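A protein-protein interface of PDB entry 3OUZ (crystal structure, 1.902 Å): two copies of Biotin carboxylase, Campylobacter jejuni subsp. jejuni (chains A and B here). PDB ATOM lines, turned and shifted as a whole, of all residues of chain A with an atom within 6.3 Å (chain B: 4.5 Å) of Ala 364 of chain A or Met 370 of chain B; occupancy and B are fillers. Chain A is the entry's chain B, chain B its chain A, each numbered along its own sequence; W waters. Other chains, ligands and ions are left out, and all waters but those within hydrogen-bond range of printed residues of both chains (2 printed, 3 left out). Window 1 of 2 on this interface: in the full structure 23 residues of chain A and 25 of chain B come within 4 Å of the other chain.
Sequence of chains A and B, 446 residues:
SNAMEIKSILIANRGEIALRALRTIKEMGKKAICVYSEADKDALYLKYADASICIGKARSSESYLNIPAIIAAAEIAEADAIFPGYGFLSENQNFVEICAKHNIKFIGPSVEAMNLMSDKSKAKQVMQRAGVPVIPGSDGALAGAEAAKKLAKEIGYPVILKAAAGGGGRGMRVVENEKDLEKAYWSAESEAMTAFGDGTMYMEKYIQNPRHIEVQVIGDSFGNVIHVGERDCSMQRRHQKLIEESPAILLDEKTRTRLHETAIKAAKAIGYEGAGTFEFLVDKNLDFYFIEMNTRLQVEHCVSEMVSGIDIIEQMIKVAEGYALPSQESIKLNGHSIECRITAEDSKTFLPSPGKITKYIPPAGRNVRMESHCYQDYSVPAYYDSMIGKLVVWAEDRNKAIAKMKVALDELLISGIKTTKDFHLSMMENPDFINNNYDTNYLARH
Among the printed residues, Asp or Glu carboxylates within 4 Å of a Lys or Arg side-chain nitrogen of the other chain: Glu 411 of chain A with Arg 23 of chain B.
Positions printed for both chains: 362, 363 and 368.
Of the 6 pairs that touch across the chains among the printed residues, none has its exchanged pair printed and touching as well.
Of the printed residues of chain A, Met 370 of chain B touches Ala 364.
Of the printed residues of chain A, Glu 371 of chain B touches Gly 365.
Printed residues of chain B within 4 Å of Gly 365 of chain A: Arg 23 (3.8 Å) and Glu 371 (3.9 Å).
Of the printed residues of chain A, Arg 369 of chain B touches Arg 366 (3.7 Å).
Of the printed residues of chain B, Glu 411 of chain A touches Arg 23 (3.0 Å).
Of the printed residues of chain B, Arg 366 of chain A touches Arg 369.
Pro 362 of chain B touches none of the printed residues of chain A.
Leu 391 of chain B touches none of the printed residues of chain A.
The nearest printed residue of chain B that does not touch Ala 364 of chain A is Glu 371 of chain B (5.6 Å).
The nearest printed residue of chain A that does not touch Met 370 of chain B is Gly 365 of chain A (4.9 Å).
Among the printed residues, pairs that only touch across the chains: Ala 364 of chain A with Arg 23 of chain B (3.5 Å), Ala 364 of chain A with Met 370 of chain B (3.8 Å), Gly 365 of chain A with Arg 23 of chain B (3.8 Å), Gly 365 of chain A with Glu 371 of chain B (3.9 Å) and Arg 366 of chain A with Arg 369 of chain B (3.7 Å).
The guanidinium group of Arg 23 of chain B lies within salt-bridge range of the side-chain carboxylate of Glu 411 of chain A (3.0 Å).
NE of Arg 369 of chain B is in salt-bridge range of OE2 of Glu 371 of chain B, 2.7 Å away.
N of Glu 371 of chain B is in hydrogen-bond range of O of Lys 390 of chain B.
Water W2 lies within hydrogen-bond range of N of Gly 365 of chain A, OE2 of Glu 371 of chain B and O of Met 370 of chain B.
Water W1 lies within hydrogen-bond range of O of Pro 362 of chain A (2.9 Å) and NH2 of Arg 23 of chain B (3.3 Å).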
ATOM      1  N   PRO A 362     -19.723 -18.953  -9.967  1.00  0.00           N
ATOM      2  CA  PRO A 362     -18.722 -18.919 -11.036  1.00  0.00           C
ATOM      3  C   PRO A 362     -18.569 -17.497 -11.574  1.00  0.00           C
ATOM      4  O   PRO A 362     -19.477 -16.672 -11.398  1.00  0.00           O
ATOM      5  CB  PRO A 362     -19.325 -19.847 -12.104  1.00  0.00           C
ATOM      6  CG  PRO A 362     -20.780 -19.787 -11.873  1.00  0.00           C
ATOM      7  CD  PRO A 362     -20.996 -19.549 -10.403  1.00  0.00           C
ATOM      8  N   PRO A 363     -17.433 -17.194 -12.209  1.00  0.00           N
ATOM      9  CA  PRO A 363     -17.357 -15.869 -12.830  1.00  0.00           C
ATOM     10  C   PRO A 363     -18.096 -15.909 -14.152  1.00  0.00           C
ATOM     11  O   PRO A 363     -18.398 -16.998 -14.663  1.00  0.00           O
ATOM     12  CB  PRO A 363     -15.863 -15.682 -13.084  1.00  0.00           C
ATOM     13  CG  PRO A 363     -15.362 -17.053 -13.298  1.00  0.00           C
ATOM     14  CD  PRO A 363     -16.189 -17.963 -12.388  1.00  0.00           C
ATOM     15  N   ALA A 364     -18.377 -14.731 -14.690  1.00  0.00           N
ATOM     16  CA  ALA A 364     -19.073 -14.597 -15.956  1.00  0.00           C
ATOM     17  C   ALA A 364     -18.616 -13.274 -16.541  1.00  0.00           C
ATOM     18  O   ALA A 364     -17.647 -12.693 -16.085  1.00  0.00           O
ATOM     19  CB  ALA A 364     -20.607 -14.605 -15.742  1.00  0.00           C
ATOM     20  N   GLY A 365     -19.312 -12.786 -17.546  1.00  0.00           N
ATOM     21  CA  GLY A 365     -18.911 -11.537 -18.150  1.00  0.00           C
ATOM     22  C   GLY A 365     -18.471 -11.753 -19.577  1.00  0.00           C
ATOM     23  O   GLY A 365     -18.396 -12.871 -20.073  1.00  0.00           O
ATOM     24  N   ARG A 366     -18.180 -10.645 -20.227  1.00  0.00           N
ATOM     25  CA  ARG A 366     -17.772 -10.606 -21.606  1.00  0.00           C
ATOM     26  C   ARG A 366     -16.515 -11.461 -21.826  1.00  0.00           C
ATOM     27  O   ARG A 366     -15.502 -11.254 -21.174  1.00  0.00           O
ATOM     28  CB  ARG A 366     -17.508  -9.118 -21.961  1.00  0.00           C
ATOM     29  CG  ARG A 366     -17.005  -8.885 -23.374  1.00  0.00           C
ATOM     30  CD  ARG A 366     -16.989  -7.376 -23.752  1.00  0.00           C
ATOM     31  NE  ARG A 366     -16.245  -7.238 -25.003  1.00  0.00           N
ATOM     32  CZ  ARG A 366     -14.932  -7.057 -25.077  1.00  0.00           C
ATOM     33  NH1 ARG A 366     -14.201  -6.947 -23.968  1.00  0.00           N
ATOM     34  NH2 ARG A 366     -14.348  -6.986 -26.265  1.00  0.00           N
ATOM     35  N   VAL A 368     -15.642 -14.429 -21.028  1.00  0.00           N
ATOM     36  CA  VAL A 368     -15.231 -15.275 -19.919  1.00  0.00           C
ATOM     37  C   VAL A 368     -16.021 -16.567 -20.062  1.00  0.00           C
ATOM     38  O   VAL A 368     -17.250 -16.560 -20.157  1.00  0.00           O
ATOM     39  CB  VAL A 368     -15.553 -14.611 -18.564  1.00  0.00           C
ATOM     40  CG1 VAL A 368     -15.300 -15.569 -17.409  1.00  0.00           C
ATOM     41  CG2 VAL A 368     -14.712 -13.339 -18.400  1.00  0.00           C
ATOM     42  N   ALA A 408     -11.679 -12.466 -13.305  1.00  0.00           N
ATOM     43  CA  ALA A 408     -12.513 -13.661 -13.313  1.00  0.00           C
ATOM     44  C   ALA A 408     -12.155 -14.577 -12.152  1.00  0.00           C
ATOM     45  O   ALA A 408     -13.039 -15.114 -11.482  1.00  0.00           O
ATOM     46  CB  ALA A 408     -12.385 -14.402 -14.654  1.00  0.00           C
ATOM     47  N   GLU A 411     -13.509 -13.291  -8.961  1.00  0.00           N
ATOM     48  CA  GLU A 411     -14.956 -13.432  -8.812  1.00  0.00           C
ATOM     49  C   GLU A 411     -15.440 -14.874  -8.620  1.00  0.00           C
ATOM     50  O   GLU A 411     -16.580 -15.106  -8.233  1.00  0.00           O
ATOM     51  CB  GLU A 411     -15.662 -12.713  -9.958  1.00  0.00           C
ATOM     52  CG  GLU A 411     -15.254 -11.217  -9.886  1.00  0.00           C
ATOM     53  CD  GLU A 411     -15.966 -10.326 -10.868  1.00  0.00           C
ATOM     54  OE1 GLU A 411     -16.726 -10.875 -11.696  1.00  0.00           O
ATOM     55  OE2 GLU A 411     -15.765  -9.073 -10.797  1.00  0.00           O
ATOM     56  N   ARG B  23     -17.077  -5.094 -13.622  1.00  0.00           N
ATOM     57  CA  ARG B  23     -16.130  -5.961 -14.311  1.00  0.00           C
ATOM     58  C   ARG B  23     -15.227  -5.201 -15.277  1.00  0.00           C
ATOM     59  O   ARG B  23     -14.011  -5.371 -15.262  1.00  0.00           O
ATOM     60  CB  ARG B  23     -16.858  -7.107 -15.018  1.00  0.00           C
ATOM     61  CG  ARG B  23     -17.471  -8.070 -14.039  1.00  0.00           C
ATOM     62  CD  ARG B  23     -18.369  -9.078 -14.764  1.00  0.00           C
ATOM     63  NE  ARG B  23     -18.712 -10.162 -13.862  1.00  0.00           N
ATOM     64  CZ  ARG B  23     -19.844 -10.857 -13.938  1.00  0.00           C
ATOM     65  NH1 ARG B  23     -20.739 -10.565 -14.864  1.00  0.00           N
ATOM     66  NH2 ARG B  23     -20.072 -11.841 -13.084  1.00  0.00           N
ATOM     67  N   TYR B 360     -29.669 -22.291  -7.933  1.00  0.00           N
ATOM     68  CA  TYR B 360     -29.272 -21.426  -9.026  1.00  0.00           C
ATOM     69  C   TYR B 360     -28.087 -22.022  -9.765  1.00  0.00           C
ATOM     70  O   TYR B 360     -26.975 -22.056  -9.241  1.00  0.00           O
ATOM     71  CB  TYR B 360     -28.936 -20.013  -8.525  1.00  0.00           C
ATOM     72  CG  TYR B 360     -28.629 -19.069  -9.660  1.00  0.00           C
ATOM     73  CD1 TYR B 360     -29.652 -18.577 -10.460  1.00  0.00           C
ATOM     74  CD2 TYR B 360     -27.319 -18.684  -9.950  1.00  0.00           C
ATOM     75  CE1 TYR B 360     -29.394 -17.719 -11.512  1.00  0.00           C
ATOM     76  CE2 TYR B 360     -27.044 -17.811 -11.011  1.00  0.00           C
ATOM     77  CZ  TYR B 360     -28.102 -17.342 -11.787  1.00  0.00           C
ATOM     78  OH  TYR B 360     -27.882 -16.492 -12.842  1.00  0.00           O
ATOM     79  N   PRO B 362     -26.490 -21.399 -13.490  1.00  0.00           N
ATOM     80  CA  PRO B 362     -26.617 -20.640 -14.734  1.00  0.00           C
ATOM     81  C   PRO B 362     -26.098 -21.424 -15.923  1.00  0.00           C
ATOM     82  O   PRO B 362     -25.265 -22.321 -15.767  1.00  0.00           O
ATOM     83  CB  PRO B 362     -25.717 -19.423 -14.489  1.00  0.00           C
ATOM     84  CG  PRO B 362     -24.657 -19.932 -13.565  1.00  0.00           C
ATOM     85  CD  PRO B 362     -25.386 -20.904 -12.649  1.00  0.00           C
ATOM     86  N   PRO B 363     -26.580 -21.090 -17.122  1.00  0.00           N
ATOM     87  CA  PRO B 363     -26.008 -21.749 -18.297  1.00  0.00           C
ATOM     88  C   PRO B 363     -24.617 -21.179 -18.540  1.00  0.00           C
ATOM     89  O   PRO B 363     -24.293 -20.105 -18.033  1.00  0.00           O
ATOM     90  CB  PRO B 363     -26.936 -21.307 -19.431  1.00  0.00           C
ATOM     91  CG  PRO B 363     -27.456 -20.002 -18.995  1.00  0.00           C
ATOM     92  CD  PRO B 363     -27.563 -20.052 -17.479  1.00  0.00           C
ATOM     93  N   VAL B 368     -21.924 -18.021 -24.795  1.00  0.00           N
ATOM     94  CA  VAL B 368     -23.091 -17.844 -23.950  1.00  0.00           C
ATOM     95  C   VAL B 368     -22.700 -16.909 -22.832  1.00  0.00           C
ATOM     96  O   VAL B 368     -21.706 -17.143 -22.160  1.00  0.00           O
ATOM     97  CB  VAL B 368     -23.541 -19.190 -23.354  1.00  0.00           C
ATOM     98  CG1 VAL B 368     -24.650 -18.979 -22.299  1.00  0.00           C
ATOM     99  CG2 VAL B 368     -24.037 -20.091 -24.468  1.00  0.00           C
ATOM    100  N   ARG B 369     -23.480 -15.851 -22.644  1.00  0.00           N
ATOM    101  CA  ARG B 369     -23.187 -14.829 -21.662  1.00  0.00           C
ATOM    102  C   ARG B 369     -24.426 -14.608 -20.781  1.00  0.00           C
ATOM    103  O   ARG B 369     -25.415 -14.022 -21.234  1.00  0.00           O
ATOM    104  CB  ARG B 369     -22.823 -13.551 -22.433  1.00  0.00           C
ATOM    105  CG  ARG B 369     -22.089 -12.512 -21.663  1.00  0.00           C
ATOM    106  CD  ARG B 369     -21.600 -11.370 -22.572  1.00  0.00           C
ATOM    107  NE  ARG B 369     -21.523 -10.150 -21.779  1.00  0.00           N
ATOM    108  CZ  ARG B 369     -21.258  -8.949 -22.271  1.00  0.00           C
ATOM    109  NH1 ARG B 369     -21.009  -8.804 -23.567  1.00  0.00           N
ATOM    110  NH2 ARG B 369     -21.218  -7.901 -21.454  1.00  0.00           N
ATOM    111  N   MET B 370     -24.368 -15.069 -19.537  1.00  0.00           N
ATOM    112  CA  MET B 370     -25.454 -14.845 -18.586  1.00  0.00           C
ATOM    113  C   MET B 370     -25.061 -13.640 -17.739  1.00  0.00           C
ATOM    114  O   MET B 370     -24.093 -13.725 -16.972  1.00  0.00           O
ATOM    115  CB  MET B 370     -25.662 -16.104 -17.708  1.00  0.00           C
ATOM    116  CG  MET B 370     -26.707 -15.958 -16.578  1.00  0.00           C
ATOM    117  SD  MET B 370     -28.496 -15.477 -17.271  1.00  0.00           S
ATOM    118  CE  MET B 370     -29.666 -15.776 -15.695  1.00  0.00           C
ATOM    119  N   GLU B 371     -25.768 -12.513 -17.923  1.00  0.00           N
ATOM    120  CA  GLU B 371     -25.489 -11.283 -17.207  1.00  0.00           C
ATOM    121  C   GLU B 371     -26.450 -11.204 -16.024  1.00  0.00           C
ATOM    122  O   GLU B 371     -27.624 -10.859 -16.186  1.00  0.00           O
ATOM    123  CB  GLU B 371     -25.707 -10.075 -18.138  1.00  0.00           C
ATOM    124  CG  GLU B 371     -24.708 -10.018 -19.295  1.00  0.00           C
ATOM    125  CD  GLU B 371     -23.351  -9.430 -18.851  1.00  0.00           C
ATOM    126  OE1 GLU B 371     -23.346  -8.411 -18.135  1.00  0.00           O
ATOM    127  OE2 GLU B 371     -22.301  -9.990 -19.203  1.00  0.00           O
ATOM    128  N   SER B 372     -25.957 -11.536 -14.840  1.00  0.00           N
ATOM    129  CA  SER B 372     -26.815 -11.625 -13.667  1.00  0.00           C
ATOM    130  C   SER B 372     -26.034 -11.417 -12.394  1.00  0.00           C
ATOM    131  O   SER B 372     -24.898 -11.868 -12.292  1.00  0.00           O
ATOM    132  CB  SER B 372     -27.449 -13.014 -13.592  1.00  0.00           C
ATOM    133  OG  SER B 372     -28.209 -13.145 -12.397  1.00  0.00           O
ATOM    134  N   ILE B 388     -33.752 -11.010 -13.053  1.00  0.00           N
ATOM    135  CA  ILE B 388     -32.876 -12.060 -12.559  1.00  0.00           C
ATOM    136  C   ILE B 388     -31.557 -11.935 -13.341  1.00  0.00           C
ATOM    137  O   ILE B 388     -30.477 -11.828 -12.759  1.00  0.00           O
ATOM    138  CB  ILE B 388     -33.501 -13.460 -12.746  1.00  0.00           C
ATOM    139  CG1 ILE B 388     -34.648 -13.649 -11.748  1.00  0.00           C
ATOM    140  CG2 ILE B 388     -32.473 -14.548 -12.536  1.00  0.00           C
ATOM    141  CD1 ILE B 388     -35.381 -14.954 -11.924  1.00  0.00           C
ATOM    142  N   GLY B 389     -31.661 -11.917 -14.665  1.00  0.00           N
ATOM    143  CA  GLY B 389     -30.494 -11.711 -15.502  1.00  0.00           C
ATOM    144  C   GLY B 389     -30.834 -11.673 -16.974  1.00  0.00           C
ATOM    145  O   GLY B 389     -31.957 -11.982 -17.378  1.00  0.00           O
ATOM    146  N   LYS B 390     -29.865 -11.270 -17.783  1.00  0.00           N
ATOM    147  CA  LYS B 390     -30.056 -11.248 -19.221  1.00  0.00           C
ATOM    148  C   LYS B 390     -29.234 -12.396 -19.786  1.00  0.00           C
ATOM    149  O   LYS B 390     -28.031 -12.501 -19.538  1.00  0.00           O
ATOM    150  CB  LYS B 390     -29.588  -9.906 -19.803  1.00  0.00           C
ATOM    151  CG  LYS B 390     -30.286  -8.715 -19.160  1.00  0.00           C
ATOM    152  CD  LYS B 390     -29.675  -7.390 -19.590  1.00  0.00           C
ATOM    153  CE  LYS B 390     -28.208  -7.285 -19.250  1.00  0.00           C
ATOM    154  NZ  LYS B 390     -27.805  -5.854 -19.387  1.00  0.00           N
ATOM    155  N   LEU B 391     -29.882 -13.269 -20.542  1.00  0.00           N
ATOM    156  CA  LEU B 391     -29.160 -14.388 -21.134  1.00  0.00           C
ATOM    157  C   LEU B 391     -28.889 -13.985 -22.575  1.00  0.00           C
ATOM    158  O   LEU B 391     -29.816 -13.679 -23.323  1.00  0.00           O
ATOM    159  CB  LEU B 391     -30.012 -15.659 -21.059  1.00  0.00           C
ATOM    160  CG  LEU B 391     -29.416 -16.943 -21.636  1.00  0.00           C
ATOM    161  CD1 LEU B 391     -27.999 -17.196 -21.064  1.00  0.00           C
ATOM    162  CD2 LEU B 391     -30.348 -18.141 -21.377  1.00  0.00           C
ATOM    163  N   LEU B 412     -30.502 -23.428 -17.709  1.00  0.00           N
ATOM    164  CA  LEU B 412     -30.711 -22.503 -16.596  1.00  0.00           C
ATOM    165  C   LEU B 412     -31.635 -23.150 -15.559  1.00  0.00           C
ATOM    166  O   LEU B 412     -32.798 -23.441 -15.844  1.00  0.00           O
ATOM    167  CB  LEU B 412     -31.313 -21.186 -17.105  1.00  0.00           C
ATOM    168  CG  LEU B 412     -31.770 -20.175 -16.038  1.00  0.00           C
ATOM    169  CD1 LEU B 412     -30.583 -19.669 -15.196  1.00  0.00           C
ATOM    170  CD2 LEU B 412     -32.493 -19.012 -16.717  1.00  0.00           C
HETATM  171  O   HOH W   1     -19.304 -13.843 -10.580  1.00  0.00           O
HETATM  172  O   HOH W   2     -21.923 -12.612 -18.390  1.00  0.00           O
